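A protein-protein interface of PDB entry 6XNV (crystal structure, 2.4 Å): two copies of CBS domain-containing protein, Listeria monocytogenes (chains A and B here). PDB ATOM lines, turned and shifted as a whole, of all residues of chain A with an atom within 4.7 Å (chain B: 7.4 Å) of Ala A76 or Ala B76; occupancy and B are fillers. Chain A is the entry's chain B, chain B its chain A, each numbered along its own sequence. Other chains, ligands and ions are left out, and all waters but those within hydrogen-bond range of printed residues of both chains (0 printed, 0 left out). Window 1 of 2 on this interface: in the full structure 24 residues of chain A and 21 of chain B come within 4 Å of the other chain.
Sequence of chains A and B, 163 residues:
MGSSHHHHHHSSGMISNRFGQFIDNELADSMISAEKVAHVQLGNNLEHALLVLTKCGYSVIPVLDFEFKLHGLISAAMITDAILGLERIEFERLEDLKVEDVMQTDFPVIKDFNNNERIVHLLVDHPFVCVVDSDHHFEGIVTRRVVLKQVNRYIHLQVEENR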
ATOM      1  N   LEU A  50     -38.557 -22.620 -13.131  1.00  0.00           N
ATOM      2  CA  LEU A  50     -37.608 -23.727 -13.193  1.00  0.00           C
ATOM      3  C   LEU A  50     -37.692 -24.446 -14.530  1.00  0.00           C
ATOM      4  O   LEU A  50     -36.664 -24.829 -15.103  1.00  0.00           O
ATOM      5  CB  LEU A  50     -37.862 -24.712 -12.056  1.00  0.00           C
ATOM      6  CG  LEU A  50     -36.879 -24.759 -10.891  1.00  0.00           C
ATOM      7  CD1 LEU A  50     -36.984 -26.120 -10.245  1.00  0.00           C
ATOM      8  CD2 LEU A  50     -35.416 -24.451 -11.292  1.00  0.00           C
ATOM      9  N   LEU A  53     -36.017 -22.300 -17.139  1.00  0.00           N
ATOM     10  CA  LEU A  53     -34.576 -22.369 -16.918  1.00  0.00           C
ATOM     11  C   LEU A  53     -34.036 -23.691 -17.429  1.00  0.00           C
ATOM     12  O   LEU A  53     -33.059 -23.725 -18.194  1.00  0.00           O
ATOM     13  CB  LEU A  53     -34.250 -22.183 -15.432  1.00  0.00           C
ATOM     14  CG  LEU A  53     -34.281 -20.760 -14.873  1.00  0.00           C
ATOM     15  CD1 LEU A  53     -34.433 -20.802 -13.366  1.00  0.00           C
ATOM     16  CD2 LEU A  53     -33.010 -20.009 -15.251  1.00  0.00           C
ATOM     17  N   SER A  59     -28.172 -20.360 -17.316  1.00  0.00           N
ATOM     18  CA  SER A  59     -28.179 -20.376 -15.856  1.00  0.00           C
ATOM     19  C   SER A  59     -28.791 -19.122 -15.244  1.00  0.00           C
ATOM     20  O   SER A  59     -29.326 -19.194 -14.132  1.00  0.00           O
ATOM     21  CB  SER A  59     -26.756 -20.556 -15.309  1.00  0.00           C
ATOM     22  OG  SER A  59     -25.942 -19.491 -15.754  1.00  0.00           O
ATOM     23  N   SER A  75     -32.465 -17.315 -11.506  1.00  0.00           N
ATOM     24  CA  SER A  75     -31.678 -18.527 -11.657  1.00  0.00           C
ATOM     25  C   SER A  75     -32.268 -19.635 -10.786  1.00  0.00           C
ATOM     26  O   SER A  75     -33.087 -19.387  -9.889  1.00  0.00           O
ATOM     27  CB  SER A  75     -30.218 -18.290 -11.272  1.00  0.00           C
ATOM     28  OG  SER A  75     -30.139 -18.022  -9.875  1.00  0.00           O
ATOM     29  N   ALA A  76     -31.809 -20.865 -11.039  1.00  0.00           N
ATOM     30  CA  ALA A  76     -32.205 -22.005 -10.208  1.00  0.00           C
ATOM     31  C   ALA A  76     -31.776 -21.817  -8.759  1.00  0.00           C
ATOM     32  O   ALA A  76     -32.527 -22.148  -7.835  1.00  0.00           O
ATOM     33  CB  ALA A  76     -31.616 -23.309 -10.756  1.00  0.00           C
ATOM     34  N   ALA A  77     -30.572 -21.285  -8.538  1.00  0.00           N
ATOM     35  CA  ALA A  77     -30.102 -21.066  -7.175  1.00  0.00           C
ATOM     36  C   ALA A  77     -30.998 -20.073  -6.421  1.00  0.00           C
ATOM     37  O   ALA A  77     -31.230 -20.226  -5.213  1.00  0.00           O
ATOM     38  CB  ALA A  77     -28.640 -20.598  -7.197  1.00  0.00           C
ATOM     39  N   MET A  78     -31.524 -19.055  -7.106  1.00  0.00           N
ATOM     40  CA  MET A  78     -32.440 -18.147  -6.412  1.00  0.00           C
ATOM     41  C   MET A  78     -33.691 -18.888  -5.960  1.00  0.00           C
ATOM     42  O   MET A  78     -34.195 -18.674  -4.847  1.00  0.00           O
ATOM     43  CB  MET A  78     -32.816 -16.963  -7.310  1.00  0.00           C
ATOM     44  CG  MET A  78     -31.649 -16.012  -7.678  1.00  0.00           C
ATOM     45  SD  MET A  78     -32.221 -14.728  -8.826  1.00  0.00           S
ATOM     46  CE  MET A  78     -30.772 -14.411  -9.816  1.00  0.00           C
ATOM     47  N   ILE A  79     -34.194 -19.773  -6.818  1.00  0.00           N
ATOM     48  CA  ILE A  79     -35.411 -20.511  -6.531  1.00  0.00           C
ATOM     49  C   ILE A  79     -35.169 -21.509  -5.404  1.00  0.00           C
ATOM     50  O   ILE A  79     -35.919 -21.565  -4.422  1.00  0.00           O
ATOM     51  CB  ILE A  79     -35.903 -21.198  -7.818  1.00  0.00           C
ATOM     52  CG1 ILE A  79     -36.132 -20.163  -8.928  1.00  0.00           C
ATOM     53  CG2 ILE A  79     -37.158 -21.968  -7.572  1.00  0.00           C
ATOM     54  CD1 ILE A  79     -36.659 -20.762 -10.242  1.00  0.00           C
ATOM     55  N   THR A  80     -34.090 -22.277  -5.501  1.00  0.00           N
ATOM     56  CA  THR A  80     -33.825 -23.309  -4.512  1.00  0.00           C
ATOM     57  C   THR A  80     -33.554 -22.706  -3.142  1.00  0.00           C
ATOM     58  O   THR A  80     -34.028 -23.216  -2.118  1.00  0.00           O
ATOM     59  CB  THR A  80     -32.648 -24.146  -4.974  1.00  0.00           C
ATOM     60  OG1 THR A  80     -32.908 -24.577  -6.314  1.00  0.00           O
ATOM     61  CG2 THR A  80     -32.448 -25.358  -4.057  1.00  0.00           C
ATOM     62  N   ALA B  49     -25.859 -32.412  -4.203  1.00  0.00           N
ATOM     63  CA  ALA B  49     -25.266 -31.524  -5.194  1.00  0.00           C
ATOM     64  C   ALA B  49     -26.039 -30.210  -5.298  1.00  0.00           C
ATOM     65  O   ALA B  49     -25.434 -29.138  -5.411  1.00  0.00           O
ATOM     66  CB  ALA B  49     -25.188 -32.223  -6.549  1.00  0.00           C
ATOM     67  N   LEU B  50     -27.374 -30.262  -5.235  1.00  0.00           N
ATOM     68  CA  LEU B  50     -28.147 -29.020  -5.279  1.00  0.00           C
ATOM     69  C   LEU B  50     -27.805 -28.128  -4.094  1.00  0.00           C
ATOM     70  O   LEU B  50     -27.604 -26.920  -4.256  1.00  0.00           O
ATOM     71  CB  LEU B  50     -29.649 -29.304  -5.299  1.00  0.00           C
ATOM     72  CG  LEU B  50     -30.298 -29.473  -6.674  1.00  0.00           C
ATOM     73  CD1 LEU B  50     -31.829 -29.423  -6.567  1.00  0.00           C
ATOM     74  CD2 LEU B  50     -29.778 -28.457  -7.692  1.00  0.00           C
ATOM     75  N   LEU B  53     -24.434 -26.556  -4.721  1.00  0.00           N
ATOM     76  CA  LEU B  53     -24.567 -25.552  -5.768  1.00  0.00           C
ATOM     77  C   LEU B  53     -25.234 -24.301  -5.223  1.00  0.00           C
ATOM     78  O   LEU B  53     -24.729 -23.184  -5.385  1.00  0.00           O
ATOM     79  CB  LEU B  53     -25.361 -26.114  -6.945  1.00  0.00           C
ATOM     80  CG  LEU B  53     -24.525 -26.968  -7.904  1.00  0.00           C
ATOM     81  CD1 LEU B  53     -25.414 -27.951  -8.687  1.00  0.00           C
ATOM     82  CD2 LEU B  53     -23.624 -26.119  -8.842  1.00  0.00           C
ATOM     83  N   THR B  54     -26.357 -24.487  -4.524  1.00  0.00           N
ATOM     84  CA  THR B  54     -27.089 -23.352  -3.979  1.00  0.00           C
ATOM     85  C   THR B  54     -26.260 -22.621  -2.928  1.00  0.00           C
ATOM     86  O   THR B  54     -26.165 -21.389  -2.940  1.00  0.00           O
ATOM     87  CB  THR B  54     -28.418 -23.829  -3.396  1.00  0.00           C
ATOM     88  OG1 THR B  54     -29.120 -24.618  -4.379  1.00  0.00           O
ATOM     89  CG2 THR B  54     -29.271 -22.630  -2.970  1.00  0.00           C
ATOM     90  N   TYR B  58     -21.985 -20.810  -7.018  1.00  0.00           N
ATOM     91  CA  TYR B  58     -21.514 -21.031  -8.381  1.00  0.00           C
ATOM     92  C   TYR B  58     -22.433 -21.995  -9.108  1.00  0.00           C
ATOM     93  O   TYR B  58     -22.946 -22.946  -8.511  1.00  0.00           O
ATOM     94  CB  TYR B  58     -20.094 -21.574  -8.383  1.00  0.00           C
ATOM     95  CG  TYR B  58     -19.153 -20.573  -7.822  1.00  0.00           C
ATOM     96  CD1 TYR B  58     -18.907 -19.380  -8.501  1.00  0.00           C
ATOM     97  CD2 TYR B  58     -18.533 -20.782  -6.595  1.00  0.00           C
ATOM     98  CE1 TYR B  58     -18.053 -18.445  -7.980  1.00  0.00           C
ATOM     99  CE2 TYR B  58     -17.661 -19.837  -6.066  1.00  0.00           C
ATOM    100  CZ  TYR B  58     -17.429 -18.678  -6.773  1.00  0.00           C
ATOM    101  OH  TYR B  58     -16.572 -17.730  -6.282  1.00  0.00           O
ATOM    102  N   SER B  59     -22.644 -21.746 -10.398  1.00  0.00           N
ATOM    103  CA  SER B  59     -23.640 -22.509 -11.133  1.00  0.00           C
ATOM    104  C   SER B  59     -23.085 -23.761 -11.822  1.00  0.00           C
ATOM    105  O   SER B  59     -23.880 -24.602 -12.247  1.00  0.00           O
ATOM    106  CB  SER B  59     -24.301 -21.606 -12.166  1.00  0.00           C
ATOM    107  OG  SER B  59     -23.312 -21.001 -12.960  1.00  0.00           O
ATOM    108  N   VAL B  60     -21.764 -23.907 -11.954  1.00  0.00           N
ATOM    109  CA  VAL B  60     -21.127 -25.105 -12.506  1.00  0.00           C
ATOM    110  C   VAL B  60     -19.850 -25.355 -11.709  1.00  0.00           C
ATOM    111  O   VAL B  60     -19.007 -24.451 -11.586  1.00  0.00           O
ATOM    112  CB  VAL B  60     -20.771 -24.967 -14.005  1.00  0.00           C
ATOM    113  CG1 VAL B  60     -20.119 -26.256 -14.537  1.00  0.00           C
ATOM    114  CG2 VAL B  60     -21.969 -24.566 -14.884  1.00  0.00           C
ATOM    115  N   ILE B  74     -20.761 -30.510 -12.733  1.00  0.00           N
ATOM    116  CA  ILE B  74     -22.190 -30.624 -12.452  1.00  0.00           C
ATOM    117  C   ILE B  74     -22.820 -29.241 -12.276  1.00  0.00           C
ATOM    118  O   ILE B  74     -22.214 -28.332 -11.703  1.00  0.00           O
ATOM    119  CB  ILE B  74     -22.442 -31.501 -11.217  1.00  0.00           C
ATOM    120  CG1 ILE B  74     -23.933 -31.721 -11.043  1.00  0.00           C
ATOM    121  CG2 ILE B  74     -21.858 -30.867  -9.987  1.00  0.00           C
ATOM    122  CD1 ILE B  74     -24.281 -33.136 -10.776  1.00  0.00           C
ATOM    123  N   SER B  75     -24.024 -29.081 -12.802  1.00  0.00           N
ATOM    124  CA  SER B  75     -24.851 -27.896 -12.604  1.00  0.00           C
ATOM    125  C   SER B  75     -26.261 -28.318 -12.204  1.00  0.00           C
ATOM    126  O   SER B  75     -26.635 -29.500 -12.292  1.00  0.00           O
ATOM    127  CB  SER B  75     -24.924 -27.054 -13.873  1.00  0.00           C
ATOM    128  OG  SER B  75     -25.742 -27.710 -14.849  1.00  0.00           O
ATOM    129  N   ALA B  76     -27.045 -27.327 -11.758  1.00  0.00           N
ATOM    130  CA  ALA B  76     -28.459 -27.566 -11.456  1.00  0.00           C
ATOM    131  C   ALA B  76     -29.228 -27.881 -12.716  1.00  0.00           C
ATOM    132  O   ALA B  76     -30.186 -28.663 -12.678  1.00  0.00           O
ATOM    133  CB  ALA B  76     -29.100 -26.369 -10.758  1.00  0.00           C
ATOM    134  N   ALA B  77     -28.792 -27.304 -13.835  1.00  0.00           N
ATOM    135  CA  ALA B  77     -29.414 -27.587 -15.121  1.00  0.00           C
ATOM    136  C   ALA B  77     -29.313 -29.071 -15.462  1.00  0.00           C
ATOM    137  O   ALA B  77     -30.311 -29.694 -15.829  1.00  0.00           O
ATOM    138  CB  ALA B  77     -28.770 -26.733 -16.212  1.00  0.00           C
ATOM    139  N   MET B  78     -28.118 -29.660 -15.334  1.00  0.00           N
ATOM    140  CA  MET B  78     -27.984 -31.101 -15.579  1.00  0.00           C
ATOM    141  C   MET B  78     -28.890 -31.891 -14.648  1.00  0.00           C
ATOM    142  O   MET B  78     -29.546 -32.848 -15.061  1.00  0.00           O
ATOM    143  CB  MET B  78     -26.536 -31.567 -15.406  1.00  0.00           C
ATOM    144  CG  MET B  78     -25.504 -30.817 -16.232  1.00  0.00           C
ATOM    145  SD  MET B  78     -23.823 -31.282 -15.702  1.00  0.00           S
ATOM    146  CE  MET B  78     -22.865 -29.932 -16.381  1.00  0.00           C
ATOM    147  N   ILE B  79     -28.948 -31.487 -13.387  1.00  0.00           N
ATOM    148  CA  ILE B  79     -29.704 -32.232 -12.388  1.00  0.00           C
ATOM    149  C   ILE B  79     -31.187 -32.226 -12.731  1.00  0.00           C
ATOM    150  O   ILE B  79     -31.830 -33.278 -12.787  1.00  0.00           O
ATOM    151  CB  ILE B  79     -29.444 -31.647 -10.989  1.00  0.00           C
ATOM    152  CG1 ILE B  79     -28.044 -32.060 -10.511  1.00  0.00           C
ATOM    153  CG2 ILE B  79     -30.584 -32.023 -10.010  1.00  0.00           C
ATOM    154  CD1 ILE B  79     -27.590 -31.356  -9.243  1.00  0.00           C
ATOM    155  N   THR B  80     -31.744 -31.037 -12.974  1.00  0.00           N
ATOM    156  CA  THR B  80     -33.181 -30.896 -13.204  1.00  0.00           C
ATOM    157  C   THR B  80     -33.583 -31.516 -14.524  1.00  0.00           C
ATOM    158  O   THR B  80     -34.687 -32.053 -14.657  1.00  0.00           O
ATOM    159  CB  THR B  80     -33.582 -29.417 -13.197  1.00  0.00           C
ATOM    160  OG1 THR B  80     -32.978 -28.779 -12.077  1.00  0.00           O
ATOM    161  CG2 THR B  80     -35.057 -29.284 -13.051  1.00  0.00           C
ATOM    162  N   ASP B  81     -32.707 -31.426 -15.522  1.00  0.00           N
ATOM    163  CA  ASP B  81     -33.006 -32.065 -16.789  1.00  0.00           C
ATOM    164  C   ASP B  81     -33.075 -33.581 -16.642  1.00  0.00           C
ATOM    165  O   ASP B  81     -33.868 -34.230 -17.330  1.00  0.00           O
ATOM    166  CB  ASP B  81     -31.960 -31.672 -17.814  1.00  0.00           C
ATOM    167  CG  ASP B  81     -32.354 -32.055 -19.200  1.00  0.00           C
ATOM    168  OD1 ASP B  81     -33.193 -31.363 -19.816  1.00  0.00           O
ATOM    169  OD2 ASP B  81     -31.828 -33.088 -19.654  1.00  0.00           O
ATOM    170  N   ALA B  82     -32.281 -34.158 -15.736  1.00  0.00           N
ATOM    171  CA  ALA B  82     -32.284 -35.605 -15.558  1.00  0.00           C
ATOM    172  C   ALA B  82     -33.544 -36.119 -14.861  1.00  0.00           C
ATOM    173  O   ALA B  82     -33.837 -37.311 -14.954  1.00  0.00           O
ATOM    174  CB  ALA B  82     -31.042 -36.044 -14.774  1.00  0.00           C
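The backbone carbonyl oxygen (O) of Leu B50 lies within hydrogen-bond range of the side-chain hydroxyl (OG1) of Thr B54 (2.8 Å).
O of Ala B76 is in hydrogen-bond range of OG1 of Thr B80 (2.9 Å).
The backbone carbonyl oxygen (O) of Ala A76 sits at hydrogen-bond distance from the side-chain hydroxyl (OG1) of Thr A80, 2.9 Å away.
Among the printed residues, merely in contact across the chains: Ala A76 with Ala B76 (3.96 Å), Ala A77 with Thr B54 (3.8 Å) and Thr A80 with Thr B54 (3.4 Å).
Of chain B, only Ala B76 (3.96 Å) comes within 4 Å of Ala A76.
Ala B76 touches just one residue of chain A: Ala A76.
Printed residues of chain B within 4 Å of Thr A80: Thr B54.
Of the printed residues of chain A, Thr B54 touches Ala A77 (3.8 Å) and Thr A80 (3.4 Å).
The nearest residue of chain B that does not touch Ala A76 is Thr B54 (5.4 Å).
The nearest printed residue of chain A that does not touch Ala B76 is Ala A77 (5.7 Å).
The nearest printed residue of chain B that does not touch Ala A77 is Leu B53 (5.0 Å).
Hydrophobic or aromatic side chains of chain A within 4 Å of the printed part of chain B: Ala A76.
Along chain A the printed residues that touch a printed residue of chain B span positions 76 to 80.
Hydrophobic or aromatic side chains of chain B within 4 Å of the printed part of chain A: Ala B76.
Among the printed residues, 3 pairs touch across the chains.
Among the printed residues, no Asp or Glu carboxylate lies within 4 Å of a Lys or Arg side-chain nitrogen of the other chain.
Ala B76 touches its own counterpart, Ala A76.
Of the 3 pairs that touch across the chains among the printed residues, 1 has its exchanged pair printed and touching as well.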
